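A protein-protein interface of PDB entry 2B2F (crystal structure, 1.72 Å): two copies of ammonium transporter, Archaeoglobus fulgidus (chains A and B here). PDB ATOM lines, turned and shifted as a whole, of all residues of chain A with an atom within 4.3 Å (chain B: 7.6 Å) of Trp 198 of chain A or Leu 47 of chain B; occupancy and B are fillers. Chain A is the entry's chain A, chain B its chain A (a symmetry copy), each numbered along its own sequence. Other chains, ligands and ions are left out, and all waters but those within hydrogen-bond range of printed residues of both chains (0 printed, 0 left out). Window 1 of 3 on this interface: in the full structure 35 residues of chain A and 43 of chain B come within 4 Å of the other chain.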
ATOM      1  N   ALA A 194      -0.703  14.691 -18.325  1.00  0.00           N
ATOM      2  CA  ALA A 194      -1.866  13.812 -18.341  1.00  0.00           C
ATOM      3  C   ALA A 194      -2.545  13.754 -16.969  1.00  0.00           C
ATOM      4  O   ALA A 194      -3.778  13.714 -16.871  1.00  0.00           O
ATOM      5  CB  ALA A 194      -1.442  12.421 -18.769  1.00  0.00           C
ATOM      6  N   ALA A 195      -1.744  13.740 -15.908  1.00  0.00           N
ATOM      7  CA  ALA A 195      -2.274  13.698 -14.546  1.00  0.00           C
ATOM      8  C   ALA A 195      -3.025  14.974 -14.244  1.00  0.00           C
ATOM      9  O   ALA A 195      -4.084  14.947 -13.619  1.00  0.00           O
ATOM     10  CB  ALA A 195      -1.156  13.520 -13.549  1.00  0.00           C
ATOM     11  N   LEU A 196      -2.477  16.100 -14.686  1.00  0.00           N
ATOM     12  CA  LEU A 196      -3.131  17.384 -14.452  1.00  0.00           C
ATOM     13  C   LEU A 196      -4.428  17.519 -15.243  1.00  0.00           C
ATOM     14  O   LEU A 196      -5.367  18.176 -14.803  1.00  0.00           O
ATOM     15  CB  LEU A 196      -2.198  18.544 -14.811  1.00  0.00           C
ATOM     16  CG  LEU A 196      -0.872  18.609 -14.048  1.00  0.00           C
ATOM     17  CD1 LEU A 196      -0.145  19.886 -14.407  1.00  0.00           C
ATOM     18  CD2 LEU A 196      -1.128  18.551 -12.549  1.00  0.00           C
ATOM     19  N   LEU A 197      -4.473  16.911 -16.419  1.00  0.00           N
ATOM     20  CA  LEU A 197      -5.668  16.969 -17.241  1.00  0.00           C
ATOM     21  C   LEU A 197      -6.782  16.111 -16.662  1.00  0.00           C
ATOM     22  O   LEU A 197      -7.949  16.508 -16.675  1.00  0.00           O
ATOM     23  CB  LEU A 197      -5.349  16.499 -18.654  1.00  0.00           C
ATOM     24  CG  LEU A 197      -4.458  17.445 -19.454  1.00  0.00           C
ATOM     25  CD1 LEU A 197      -4.055  16.772 -20.756  1.00  0.00           C
ATOM     26  CD2 LEU A 197      -5.213  18.742 -19.743  1.00  0.00           C
ATOM     27  N   TRP A 198      -6.448  14.928 -16.162  1.00  0.00           N
ATOM     28  CA  TRP A 198      -7.485  14.075 -15.593  1.00  0.00           C
ATOM     29  C   TRP A 198      -8.048  14.762 -14.344  1.00  0.00           C
ATOM     30  O   TRP A 198      -9.259  14.855 -14.155  1.00  0.00           O
ATOM     31  CB  TRP A 198      -6.900  12.714 -15.226  1.00  0.00           C
ATOM     32  CG  TRP A 198      -7.925  11.656 -14.951  1.00  0.00           C
ATOM     33  CD1 TRP A 198      -9.048  11.781 -14.189  1.00  0.00           C
ATOM     34  CD2 TRP A 198      -7.872  10.279 -15.361  1.00  0.00           C
ATOM     35  NE1 TRP A 198      -9.695  10.569 -14.090  1.00  0.00           N
ATOM     36  CE2 TRP A 198      -8.993   9.629 -14.798  1.00  0.00           C
ATOM     37  CE3 TRP A 198      -6.980   9.531 -16.144  1.00  0.00           C
ATOM     38  CZ2 TRP A 198      -9.249   8.258 -14.989  1.00  0.00           C
ATOM     39  CZ3 TRP A 198      -7.234   8.164 -16.337  1.00  0.00           C
ATOM     40  CH2 TRP A 198      -8.362   7.546 -15.759  1.00  0.00           C
ATOM     41  N   PHE A 199      -7.149  15.254 -13.502  1.00  0.00           N
ATOM     42  CA  PHE A 199      -7.518  15.942 -12.272  1.00  0.00           C
ATOM     43  C   PHE A 199      -8.390  17.177 -12.556  1.00  0.00           C
ATOM     44  O   PHE A 199      -9.434  17.357 -11.936  1.00  0.00           O
ATOM     45  CB  PHE A 199      -6.228  16.327 -11.534  1.00  0.00           C
ATOM     46  CG  PHE A 199      -6.433  17.258 -10.372  1.00  0.00           C
ATOM     47  CD1 PHE A 199      -7.179  16.865  -9.264  1.00  0.00           C
ATOM     48  CD2 PHE A 199      -5.846  18.522 -10.378  1.00  0.00           C
ATOM     49  CE1 PHE A 199      -7.338  17.715  -8.177  1.00  0.00           C
ATOM     50  CE2 PHE A 199      -5.994  19.383  -9.299  1.00  0.00           C
ATOM     51  CZ  PHE A 199      -6.741  18.978  -8.193  1.00  0.00           C
ATOM     52  N   GLY A 200      -7.971  18.014 -13.498  1.00  0.00           N
ATOM     53  CA  GLY A 200      -8.738  19.205 -13.820  1.00  0.00           C
ATOM     54  C   GLY A 200     -10.095  18.924 -14.445  1.00  0.00           C
ATOM     55  O   GLY A 200     -11.015  19.739 -14.353  1.00  0.00           O
ATOM     56  N   TRP A 201     -10.228  17.765 -15.080  1.00  0.00           N
ATOM     57  CA  TRP A 201     -11.486  17.412 -15.715  1.00  0.00           C
ATOM     58  C   TRP A 201     -12.605  17.256 -14.692  1.00  0.00           C
ATOM     59  O   TRP A 201     -13.771  17.213 -15.058  1.00  0.00           O
ATOM     60  CB  TRP A 201     -11.328  16.132 -16.533  1.00  0.00           C
ATOM     61  CG  TRP A 201     -11.992  16.229 -17.878  1.00  0.00           C
ATOM     62  CD1 TRP A 201     -13.329  16.406 -18.132  1.00  0.00           C
ATOM     63  CD2 TRP A 201     -11.344  16.174 -19.154  1.00  0.00           C
ATOM     64  NE1 TRP A 201     -13.550  16.464 -19.494  1.00  0.00           N
ATOM     65  CE2 TRP A 201     -12.348  16.324 -20.143  1.00  0.00           C
ATOM     66  CE3 TRP A 201     -10.012  16.014 -19.558  1.00  0.00           C
ATOM     67  CZ2 TRP A 201     -12.057  16.317 -21.516  1.00  0.00           C
ATOM     68  CZ3 TRP A 201      -9.721  16.008 -20.923  1.00  0.00           C
ATOM     69  CH2 TRP A 201     -10.742  16.159 -21.886  1.00  0.00           C
ATOM     70  N   PHE A 202     -12.245  17.159 -13.415  1.00  0.00           N
ATOM     71  CA  PHE A 202     -13.238  17.069 -12.355  1.00  0.00           C
ATOM     72  C   PHE A 202     -13.973  18.406 -12.360  1.00  0.00           C
ATOM     73  O   PHE A 202     -15.193  18.454 -12.234  1.00  0.00           O
ATOM     74  CB  PHE A 202     -12.563  16.856 -11.001  1.00  0.00           C
ATOM     75  CG  PHE A 202     -12.289  15.417 -10.680  1.00  0.00           C
ATOM     76  CD1 PHE A 202     -13.114  14.720  -9.802  1.00  0.00           C
ATOM     77  CD2 PHE A 202     -11.222  14.751 -11.260  1.00  0.00           C
ATOM     78  CE1 PHE A 202     -12.878  13.373  -9.503  1.00  0.00           C
ATOM     79  CE2 PHE A 202     -10.980  13.406 -10.967  1.00  0.00           C
ATOM     80  CZ  PHE A 202     -11.814  12.717 -10.084  1.00  0.00           C
ATOM     81  N   ASN A 224     -15.166   9.720 -14.910  1.00  0.00           N
ATOM     82  CA  ASN A 224     -14.109   8.783 -14.545  1.00  0.00           C
ATOM     83  C   ASN A 224     -14.337   7.428 -15.204  1.00  0.00           C
ATOM     84  O   ASN A 224     -13.390   6.745 -15.599  1.00  0.00           O
ATOM     85  CB  ASN A 224     -14.051   8.628 -13.030  1.00  0.00           C
ATOM     86  CG  ASN A 224     -13.342   9.794 -12.358  1.00  0.00           C
ATOM     87  OD1 ASN A 224     -12.113   9.859 -12.356  1.00  0.00           O
ATOM     88  ND2 ASN A 224     -14.112  10.731 -11.808  1.00  0.00           N
ATOM     89  N   ALA A 227     -13.362   7.525 -18.959  1.00  0.00           N
ATOM     90  CA  ALA A 227     -11.911   7.645 -19.050  1.00  0.00           C
ATOM     91  C   ALA A 227     -11.251   6.282 -18.836  1.00  0.00           C
ATOM     92  O   ALA A 227     -10.385   5.868 -19.612  1.00  0.00           O
ATOM     93  CB  ALA A 227     -11.401   8.646 -18.013  1.00  0.00           C
ATOM     94  N   ALA A 253      -7.345   7.304 -22.350  1.00  0.00           N
ATOM     95  CA  ALA A 253      -8.110   7.876 -21.245  1.00  0.00           C
ATOM     96  C   ALA A 253      -8.690   9.227 -21.669  1.00  0.00           C
ATOM     97  O   ALA A 253      -9.857   9.526 -21.408  1.00  0.00           O
ATOM     98  CB  ALA A 253      -7.215   8.052 -20.028  1.00  0.00           C
ATOM     99  N   LEU A 257     -12.402  10.828 -21.926  1.00  0.00           N
ATOM    100  CA  LEU A 257     -12.784  12.052 -21.234  1.00  0.00           C
ATOM    101  C   LEU A 257     -13.449  13.032 -22.203  1.00  0.00           C
ATOM    102  O   LEU A 257     -14.442  13.678 -21.862  1.00  0.00           O
ATOM    103  CB  LEU A 257     -11.551  12.704 -20.582  1.00  0.00           C
ATOM    104  CG  LEU A 257     -10.957  12.010 -19.349  1.00  0.00           C
ATOM    105  CD1 LEU A 257      -9.602  12.620 -18.998  1.00  0.00           C
ATOM    106  CD2 LEU A 257     -11.924  12.143 -18.182  1.00  0.00           C
ATOM    107  N   ALA B  14     -11.477  14.836  -6.188  1.00  0.00           N
ATOM    108  CA  ALA B  14     -10.540  15.238  -7.230  1.00  0.00           C
ATOM    109  C   ALA B  14      -9.150  15.159  -6.623  1.00  0.00           C
ATOM    110  O   ALA B  14      -8.225  14.639  -7.236  1.00  0.00           O
ATOM    111  CB  ALA B  14     -10.834  16.657  -7.674  1.00  0.00           C
ATOM    112  N   VAL B  16      -8.010  13.291  -4.107  1.00  0.00           N
ATOM    113  CA  VAL B  16      -7.486  11.942  -3.881  1.00  0.00           C
ATOM    114  C   VAL B  16      -7.102  11.281  -5.203  1.00  0.00           C
ATOM    115  O   VAL B  16      -6.152  10.492  -5.264  1.00  0.00           O
ATOM    116  CB  VAL B  16      -8.502  11.055  -3.127  1.00  0.00           C
ATOM    117  CG1 VAL B  16      -7.915   9.660  -2.899  1.00  0.00           C
ATOM    118  CG2 VAL B  16      -8.841  11.700  -1.792  1.00  0.00           C
ATOM    119  N   MET B  17      -7.845  11.596  -6.264  1.00  0.00           N
ATOM    120  CA  MET B  17      -7.548  11.050  -7.589  1.00  0.00           C
ATOM    121  C   MET B  17      -6.154  11.482  -8.013  1.00  0.00           C
ATOM    122  O   MET B  17      -5.400  10.697  -8.572  1.00  0.00           O
ATOM    123  CB  MET B  17      -8.555  11.562  -8.615  1.00  0.00           C
ATOM    124  CG  MET B  17      -8.210  11.259 -10.064  1.00  0.00           C
ATOM    125  SD  MET B  17      -7.139  12.476 -10.826  1.00  0.00           S
ATOM    126  CE  MET B  17      -6.002  11.408 -11.748  1.00  0.00           C
ATOM    127  N   LEU B  18      -5.813  12.733  -7.742  1.00  0.00           N
ATOM    128  CA  LEU B  18      -4.510  13.249  -8.131  1.00  0.00           C
ATOM    129  C   LEU B  18      -3.381  12.502  -7.434  1.00  0.00           C
ATOM    130  O   LEU B  18      -2.271  12.371  -7.967  1.00  0.00           O
ATOM    131  CB  LEU B  18      -4.429  14.736  -7.803  1.00  0.00           C
ATOM    132  CG  LEU B  18      -3.134  15.438  -8.220  1.00  0.00           C
ATOM    133  CD1 LEU B  18      -2.921  15.345  -9.737  1.00  0.00           C
ATOM    134  CD2 LEU B  18      -3.213  16.896  -7.782  1.00  0.00           C
ATOM    135  N   VAL B  20      -3.046   9.405  -7.011  1.00  0.00           N
ATOM    136  CA  VAL B  20      -2.660   8.164  -7.683  1.00  0.00           C
ATOM    137  C   VAL B  20      -1.450   8.393  -8.599  1.00  0.00           C
ATOM    138  O   VAL B  20      -0.419   7.728  -8.438  1.00  0.00           O
ATOM    139  CB  VAL B  20      -3.841   7.570  -8.463  1.00  0.00           C
ATOM    140  CG1 VAL B  20      -3.444   6.230  -9.072  1.00  0.00           C
ATOM    141  CG2 VAL B  20      -5.021   7.388  -7.515  1.00  0.00           C
ATOM    142  N   PRO B  21      -1.552   9.308  -9.585  1.00  0.00           N
ATOM    143  CA  PRO B  21      -0.346   9.490 -10.408  1.00  0.00           C
ATOM    144  C   PRO B  21       0.733  10.129  -9.525  1.00  0.00           C
ATOM    145  O   PRO B  21       1.936   9.979  -9.757  1.00  0.00           O
ATOM    146  CB  PRO B  21      -0.825  10.406 -11.540  1.00  0.00           C
ATOM    147  CG  PRO B  21      -1.988  11.146 -10.936  1.00  0.00           C
ATOM    148  CD  PRO B  21      -2.691  10.058 -10.144  1.00  0.00           C
ATOM    149  N   ALA B  41       3.490   4.569 -15.232  1.00  0.00           N
ATOM    150  CA  ALA B  41       2.428   3.840 -15.923  1.00  0.00           C
ATOM    151  C   ALA B  41       1.645   2.948 -14.965  1.00  0.00           C
ATOM    152  O   ALA B  41       0.421   2.818 -15.070  1.00  0.00           O
ATOM    153  CB  ALA B  41       3.026   2.997 -17.047  1.00  0.00           C
ATOM    154  N   LEU B  42       2.358   2.324 -14.033  1.00  0.00           N
ATOM    155  CA  LEU B  42       1.714   1.449 -13.066  1.00  0.00           C
ATOM    156  C   LEU B  42       0.663   2.185 -12.258  1.00  0.00           C
ATOM    157  O   LEU B  42      -0.389   1.625 -11.945  1.00  0.00           O
ATOM    158  CB  LEU B  42       2.753   0.829 -12.126  1.00  0.00           C
ATOM    159  CG  LEU B  42       3.621  -0.285 -12.741  1.00  0.00           C
ATOM    160  CD1 LEU B  42       4.657  -0.777 -11.731  1.00  0.00           C
ATOM    161  CD2 LEU B  42       2.725  -1.438 -13.174  1.00  0.00           C
ATOM    162  N   SER B  43       0.931   3.441 -11.914  1.00  0.00           N
ATOM    163  CA  SER B  43      -0.041   4.190 -11.127  1.00  0.00           C
ATOM    164  C   SER B  43      -1.262   4.503 -11.985  1.00  0.00           C
ATOM    165  O   SER B  43      -2.395   4.432 -11.506  1.00  0.00           O
ATOM    166  CB  SER B  43       0.579   5.479 -10.568  1.00  0.00           C
ATOM    167  OG  SER B  43       0.861   6.417 -11.600  1.00  0.00           O
ATOM    168  N   PHE B  44      -1.049   4.837 -13.257  1.00  0.00           N
ATOM    169  CA  PHE B  44      -2.194   5.124 -14.113  1.00  0.00           C
ATOM    170  C   PHE B  44      -3.018   3.848 -14.328  1.00  0.00           C
ATOM    171  O   PHE B  44      -4.252   3.883 -14.343  1.00  0.00           O
ATOM    172  CB  PHE B  44      -1.758   5.691 -15.470  1.00  0.00           C
ATOM    173  CG  PHE B  44      -1.502   7.174 -15.460  1.00  0.00           C
ATOM    174  CD1 PHE B  44      -0.218   7.678 -15.287  1.00  0.00           C
ATOM    175  CD2 PHE B  44      -2.557   8.067 -15.608  1.00  0.00           C
ATOM    176  CE1 PHE B  44       0.015   9.063 -15.264  1.00  0.00           C
ATOM    177  CE2 PHE B  44      -2.338   9.449 -15.588  1.00  0.00           C
ATOM    178  CZ  PHE B  44      -1.044   9.948 -15.416  1.00  0.00           C
ATOM    179  N   ILE B  45      -2.341   2.717 -14.504  1.00  0.00           N
ATOM    180  CA  ILE B  45      -3.041   1.453 -14.691  1.00  0.00           C
ATOM    181  C   ILE B  45      -3.824   1.143 -13.415  1.00  0.00           C
ATOM    182  O   ILE B  45      -4.979   0.709 -13.467  1.00  0.00           O
ATOM    183  CB  ILE B  45      -2.036   0.331 -14.995  1.00  0.00           C
ATOM    184  CG1 ILE B  45      -1.396   0.612 -16.356  1.00  0.00           C
ATOM    185  CG2 ILE B  45      -2.721  -1.033 -14.956  1.00  0.00           C
ATOM    186  CD1 ILE B  45      -0.235  -0.282 -16.690  1.00  0.00           C
ATOM    187  N   SER B  46      -3.192   1.383 -12.270  1.00  0.00           N
ATOM    188  CA  SER B  46      -3.846   1.147 -10.995  1.00  0.00           C
ATOM    189  C   SER B  46      -5.152   1.931 -10.971  1.00  0.00           C
ATOM    190  O   SER B  46      -6.186   1.422 -10.551  1.00  0.00           O
ATOM    191  CB  SER B  46      -2.958   1.614  -9.844  1.00  0.00           C
ATOM    192  OG  SER B  46      -1.807   0.800  -9.717  1.00  0.00           O
ATOM    193  N   LEU B  47      -5.112   3.176 -11.424  1.00  0.00           N
ATOM    194  CA  LEU B  47      -6.326   3.973 -11.418  1.00  0.00           C
ATOM    195  C   LEU B  47      -7.382   3.371 -12.348  1.00  0.00           C
ATOM    196  O   LEU B  47      -8.534   3.177 -11.951  1.00  0.00           O
ATOM    197  CB  LEU B  47      -6.029   5.413 -11.851  1.00  0.00           C
ATOM    198  CG  LEU B  47      -7.243   6.351 -11.939  1.00  0.00           C
ATOM    199  CD1 LEU B  47      -7.934   6.402 -10.594  1.00  0.00           C
ATOM    200  CD2 LEU B  47      -6.801   7.747 -12.360  1.00  0.00           C
ATOM    201  N   ILE B  48      -6.979   3.071 -13.579  1.00  0.00           N
ATOM    202  CA  ILE B  48      -7.895   2.516 -14.569  1.00  0.00           C
ATOM    203  C   ILE B  48      -8.556   1.222 -14.128  1.00  0.00           C
ATOM    204  O   ILE B  48      -9.777   1.093 -14.184  1.00  0.00           O
ATOM    205  CB  ILE B  48      -7.173   2.280 -15.896  1.00  0.00           C
ATOM    206  CG1 ILE B  48      -6.725   3.630 -16.460  1.00  0.00           C
ATOM    207  CG2 ILE B  48      -8.093   1.542 -16.879  1.00  0.00           C
ATOM    208  CD1 ILE B  48      -5.854   3.523 -17.694  1.00  0.00           C
ATOM    209  N   ILE B  49      -7.749   0.268 -13.687  1.00  0.00           N
ATOM    210  CA  ILE B  49      -8.274  -1.013 -13.239  1.00  0.00           C
ATOM    211  C   ILE B  49      -9.195  -0.845 -12.030  1.00  0.00           C
ATOM    212  O   ILE B  49     -10.253  -1.471 -11.954  1.00  0.00           O
ATOM    213  CB  ILE B  49      -7.121  -1.984 -12.883  1.00  0.00           C
ATOM    214  CG1 ILE B  49      -6.239  -2.209 -14.114  1.00  0.00           C
ATOM    215  CG2 ILE B  49      -7.678  -3.309 -12.411  1.00  0.00           C
ATOM    216  CD1 ILE B  49      -6.986  -2.684 -15.347  1.00  0.00           C
ATOM    217  N   THR B  50      -8.805   0.004 -11.089  1.00  0.00           N
ATOM    218  CA  THR B  50      -9.620   0.219  -9.899  1.00  0.00           C
ATOM    219  C   THR B  50     -11.000   0.780 -10.231  1.00  0.00           C
ATOM    220  O   THR B  50     -12.021   0.303  -9.722  1.00  0.00           O
ATOM    221  CB  THR B  50      -8.906   1.150  -8.905  1.00  0.00           C
ATOM    222  OG1 THR B  50      -7.689   0.530  -8.480  1.00  0.00           O
ATOM    223  CG2 THR B  50      -9.772   1.400  -7.679  1.00  0.00           C
ATOM    224  N   VAL B  51     -11.046   1.778 -11.102  1.00  0.00           N
ATOM    225  CA  VAL B  51     -12.331   2.363 -11.468  1.00  0.00           C
ATOM    226  C   VAL B  51     -13.288   1.300 -12.013  1.00  0.00           C
ATOM    227  O   VAL B  51     -14.454   1.229 -11.613  1.00  0.00           O
ATOM    228  CB  VAL B  51     -12.177   3.475 -12.534  1.00  0.00           C
ATOM    229  CG1 VAL B  51     -13.549   3.951 -12.974  1.00  0.00           C
ATOM    230  CG2 VAL B  51     -11.392   4.654 -11.959  1.00  0.00           C
ATOM    231  N   LEU B  52     -12.787   0.472 -12.921  1.00  0.00           N
ATOM    232  CA  LEU B  52     -13.600  -0.571 -13.531  1.00  0.00           C
ATOM    233  C   LEU B  52     -14.086  -1.609 -12.524  1.00  0.00           C
ATOM    234  O   LEU B  52     -15.278  -1.900 -12.452  1.00  0.00           O
ATOM    235  CB  LEU B  52     -12.811  -1.257 -14.651  1.00  0.00           C
ATOM    236  CG  LEU B  52     -12.324  -0.318 -15.765  1.00  0.00           C
ATOM    237  CD1 LEU B  52     -11.497  -1.081 -16.787  1.00  0.00           C
ATOM    238  CD2 LEU B  52     -13.517   0.326 -16.436  1.00  0.00           C
ATOM    239  N   LEU B  53     -13.173  -2.166 -11.744  1.00  0.00           N
ATOM    240  CA  LEU B  53     -13.563  -3.173 -10.767  1.00  0.00           C
ATOM    241  C   LEU B  53     -14.499  -2.621  -9.699  1.00  0.00           C
ATOM    242  O   LEU B  53     -15.452  -3.285  -9.290  1.00  0.00           O
ATOM    243  CB  LEU B  53     -12.322  -3.770 -10.109  1.00  0.00           C
ATOM    244  CG  LEU B  53     -11.410  -4.541 -11.065  1.00  0.00           C
ATOM    245  CD1 LEU B  53     -10.202  -5.064 -10.310  1.00  0.00           C
ATOM    246  CD2 LEU B  53     -12.194  -5.690 -11.697  1.00  0.00           C
ATOM    247  N   MET B  94     -13.856   5.169  -4.169  1.00  0.00           N
ATOM    248  CA  MET B  94     -13.209   4.538  -5.300  1.00  0.00           C
ATOM    249  C   MET B  94     -11.747   4.983  -5.351  1.00  0.00           C
ATOM    250  O   MET B  94     -10.844   4.168  -5.555  1.00  0.00           O
ATOM    251  CB  MET B  94     -13.912   4.947  -6.595  1.00  0.00           C
ATOM    252  CG  MET B  94     -13.272   4.408  -7.861  1.00  0.00           C
ATOM    253  SD  MET B  94     -14.011   5.182  -9.295  1.00  0.00           S
ATOM    254  CE  MET B  94     -15.563   4.314  -9.365  1.00  0.00           C
ATOM    255  N   MET B  95     -11.522   6.280  -5.154  1.00  0.00           N
ATOM    256  CA  MET B  95     -10.174   6.844  -5.217  1.00  0.00           C
ATOM    257  C   MET B  95      -9.241   6.355  -4.107  1.00  0.00           C
ATOM    258  O   MET B  95      -8.021   6.296  -4.302  1.00  0.00           O
ATOM    259  CB  MET B  95     -10.249   8.378  -5.229  1.00  0.00           C
ATOM    260  CG  MET B  95     -11.012   8.954  -6.434  1.00  0.00           C
ATOM    261  SD  MET B  95     -10.334   8.360  -8.032  1.00  0.00           S
ATOM    262  CE  MET B  95     -11.680   8.805  -9.146  1.00  0.00           C
ATOM    263  N   ALA B  97      -9.225   3.362  -2.974  1.00  0.00           N
ATOM    264  CA  ALA B  97      -8.801   2.060  -3.455  1.00  0.00           C
ATOM    265  C   ALA B  97      -7.648   2.209  -4.426  1.00  0.00           C
ATOM    266  O   ALA B  97      -6.654   1.498  -4.333  1.00  0.00           O
ATOM    267  CB  ALA B  97      -9.961   1.361  -4.145  1.00  0.00           C
ATOM    268  N   ALA B  98      -7.797   3.139  -5.362  1.00  0.00           N
ATOM    269  CA  ALA B  98      -6.785   3.380  -6.381  1.00  0.00           C
ATOM    270  C   ALA B  98      -5.440   3.785  -5.778  1.00  0.00           C
ATOM    271  O   ALA B  98      -4.395   3.282  -6.187  1.00  0.00           O
ATOM    272  CB  ALA B  98      -7.282   4.454  -7.342  1.00  0.00           C
ATOM    273  N   VAL B  99      -5.462   4.693  -4.811  1.00  0.00           N
ATOM    274  CA  VAL B  99      -4.223   5.123  -4.182  1.00  0.00           C
ATOM    275  C   VAL B  99      -3.550   3.949  -3.488  1.00  0.00           C
ATOM    276  O   VAL B  99      -2.325   3.801  -3.536  1.00  0.00           O
ATOM    277  CB  VAL B  99      -4.480   6.220  -3.140  1.00  0.00           C
ATOM    278  CG1 VAL B  99      -3.199   6.519  -2.384  1.00  0.00           C
ATOM    279  CG2 VAL B  99      -4.992   7.485  -3.831  1.00  0.00           C
ATOM    280  N   ILE B 101      -3.628   0.723  -4.219  1.00  0.00           N
ATOM    281  CA  ILE B 101      -3.000  -0.133  -5.212  1.00  0.00           C
ATOM    282  C   ILE B 101      -1.694   0.492  -5.719  1.00  0.00           C
ATOM    283  O   ILE B 101      -0.700  -0.209  -5.908  1.00  0.00           O
ATOM    284  CB  ILE B 101      -3.974  -0.375  -6.398  1.00  0.00           C
ATOM    285  CG1 ILE B 101      -5.215  -1.120  -5.895  1.00  0.00           C
ATOM    286  CG2 ILE B 101      -3.299  -1.174  -7.498  1.00  0.00           C
ATOM    287  CD1 ILE B 101      -4.915  -2.466  -5.266  1.00  0.00           C
ATOM    288  N   ALA B 102      -1.691   1.806  -5.934  1.00  0.00           N
ATOM    289  CA  ALA B 102      -0.487   2.480  -6.413  1.00  0.00           C
ATOM    290  C   ALA B 102       0.629   2.401  -5.379  1.00  0.00           C
ATOM    291  O   ALA B 102       1.776   2.142  -5.725  1.00  0.00           O
ATOM    292  CB  ALA B 102      -0.781   3.935  -6.742  1.00  0.00           C
ATOM    293  N   PHE B 117       0.869  -7.847 -12.624  1.00  0.00           N
ATOM    294  CA  PHE B 117       0.500  -6.855 -11.618  1.00  0.00           C
ATOM    295  C   PHE B 117      -1.010  -6.614 -11.680  1.00  0.00           C
ATOM    296  O   PHE B 117      -1.683  -6.518 -10.650  1.00  0.00           O
ATOM    297  CB  PHE B 117       1.222  -5.537 -11.879  1.00  0.00           C
ATOM    298  CG  PHE B 117       0.583  -4.360 -11.199  1.00  0.00           C
ATOM    299  CD1 PHE B 117       0.648  -4.224  -9.819  1.00  0.00           C
ATOM    300  CD2 PHE B 117      -0.097  -3.397 -11.943  1.00  0.00           C
ATOM    301  CE1 PHE B 117       0.052  -3.145  -9.185  1.00  0.00           C
ATOM    302  CE2 PHE B 117      -0.703  -2.306 -11.321  1.00  0.00           C
ATOM    303  CZ  PHE B 117      -0.626  -2.179  -9.938  1.00  0.00           C
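The indole nitrogen (NE1) of Trp 198 of chain A lies within hydrogen-bond range of the side-chain amide oxygen (OD1) of Asn 224 of chain A, at 3.1 Å.
Ala 195 of chain A touches Pro 21 of chain B. Phe 44 of chain B touches Ala 195 of chain A (CZ to N, 3.9 Å). CE of Met 17 of chain B touches CG of Trp 198 of chain A (3.7 Å). CZ2 of Trp 198 of chain A touches CD2 of Leu 47 of chain B, 3.6 Å away. Phe 199 of chain A touches Ala 14 of chain B. Phe 199 of chain A touches Leu 18 of chain B. Ala 14 of chain B touches Phe 202 of chain A (CB to CG, 3.6 Å). Phe 202 of chain A touches Met 17 of chain B (CE2 to CG, 3.6 Å). O of Asn 224 of chain A touches CG1 of Val 51 of chain B (3.8 Å). Asn 224 of chain A touches Met 95 of chain B (OD1 to CE, 3.4 Å).
Of chain B, only Met 17 (3.7 Å) and Leu 47 (3.6 Å) come within 4 Å of Trp 198 of chain A. Of chain A, only Trp 198 comes within 4 Å of Leu 47 of chain B. Printed residues of chain B within 4 Å of Asn 224 of chain A: Val 51 and Met 95. Of the printed residues of chain B, Phe 199 of chain A touches Ala 14 (3.2 Å), Met 17 (3.8 Å) and Leu 18 (3.8 Å). Of the printed residues of chain A, Ala 14 of chain B touches Phe 199 and Phe 202. Printed residues of chain B within 4 Å of Phe 202 of chain A: Ala 14 and Met 17. Ser 46 of chain B touches none of the printed residues of chain A. Leu 197 of chain A touches none of the printed residues of chain B. The nearest residue of chain B that does not touch Trp 198 of chain A is Ile 48 of chain B (4.3 Å). The nearest printed residue of chain A that does not touch Leu 47 of chain B is Asn 224 of chain A (5.7 Å).
Printed residues of chain A that touch a printed residue of chain B: Ala 195, Trp 198, Phe 199, Phe 202 and Asn 224. Printed residues of chain B that touch a printed residue of chain A: Ala 14, Met 17, Leu 18, Pro 21, Phe 44, Leu 47, Val 51 and Met 95. Hydrophobic or aromatic side chains of chain B that line the printed part of chain A: Ala 14, Met 17, Leu 18, Pro 21, Phe 44, Leu 47, Val 51 and Met 95. Along chain B the printed residues that touch a printed residue of chain A span positions 14 to 95. Among the printed residues, 11 pairs touch across the chains. Among the printed residues, no Asp or Glu carboxylate lies within 4 Å of a Lys or Arg side-chain nitrogen of the other chain.
No position is printed for both chains. Of the 11 pairs that touch across the chains among the printed residues, none has its exchanged pair printed and touching as well.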
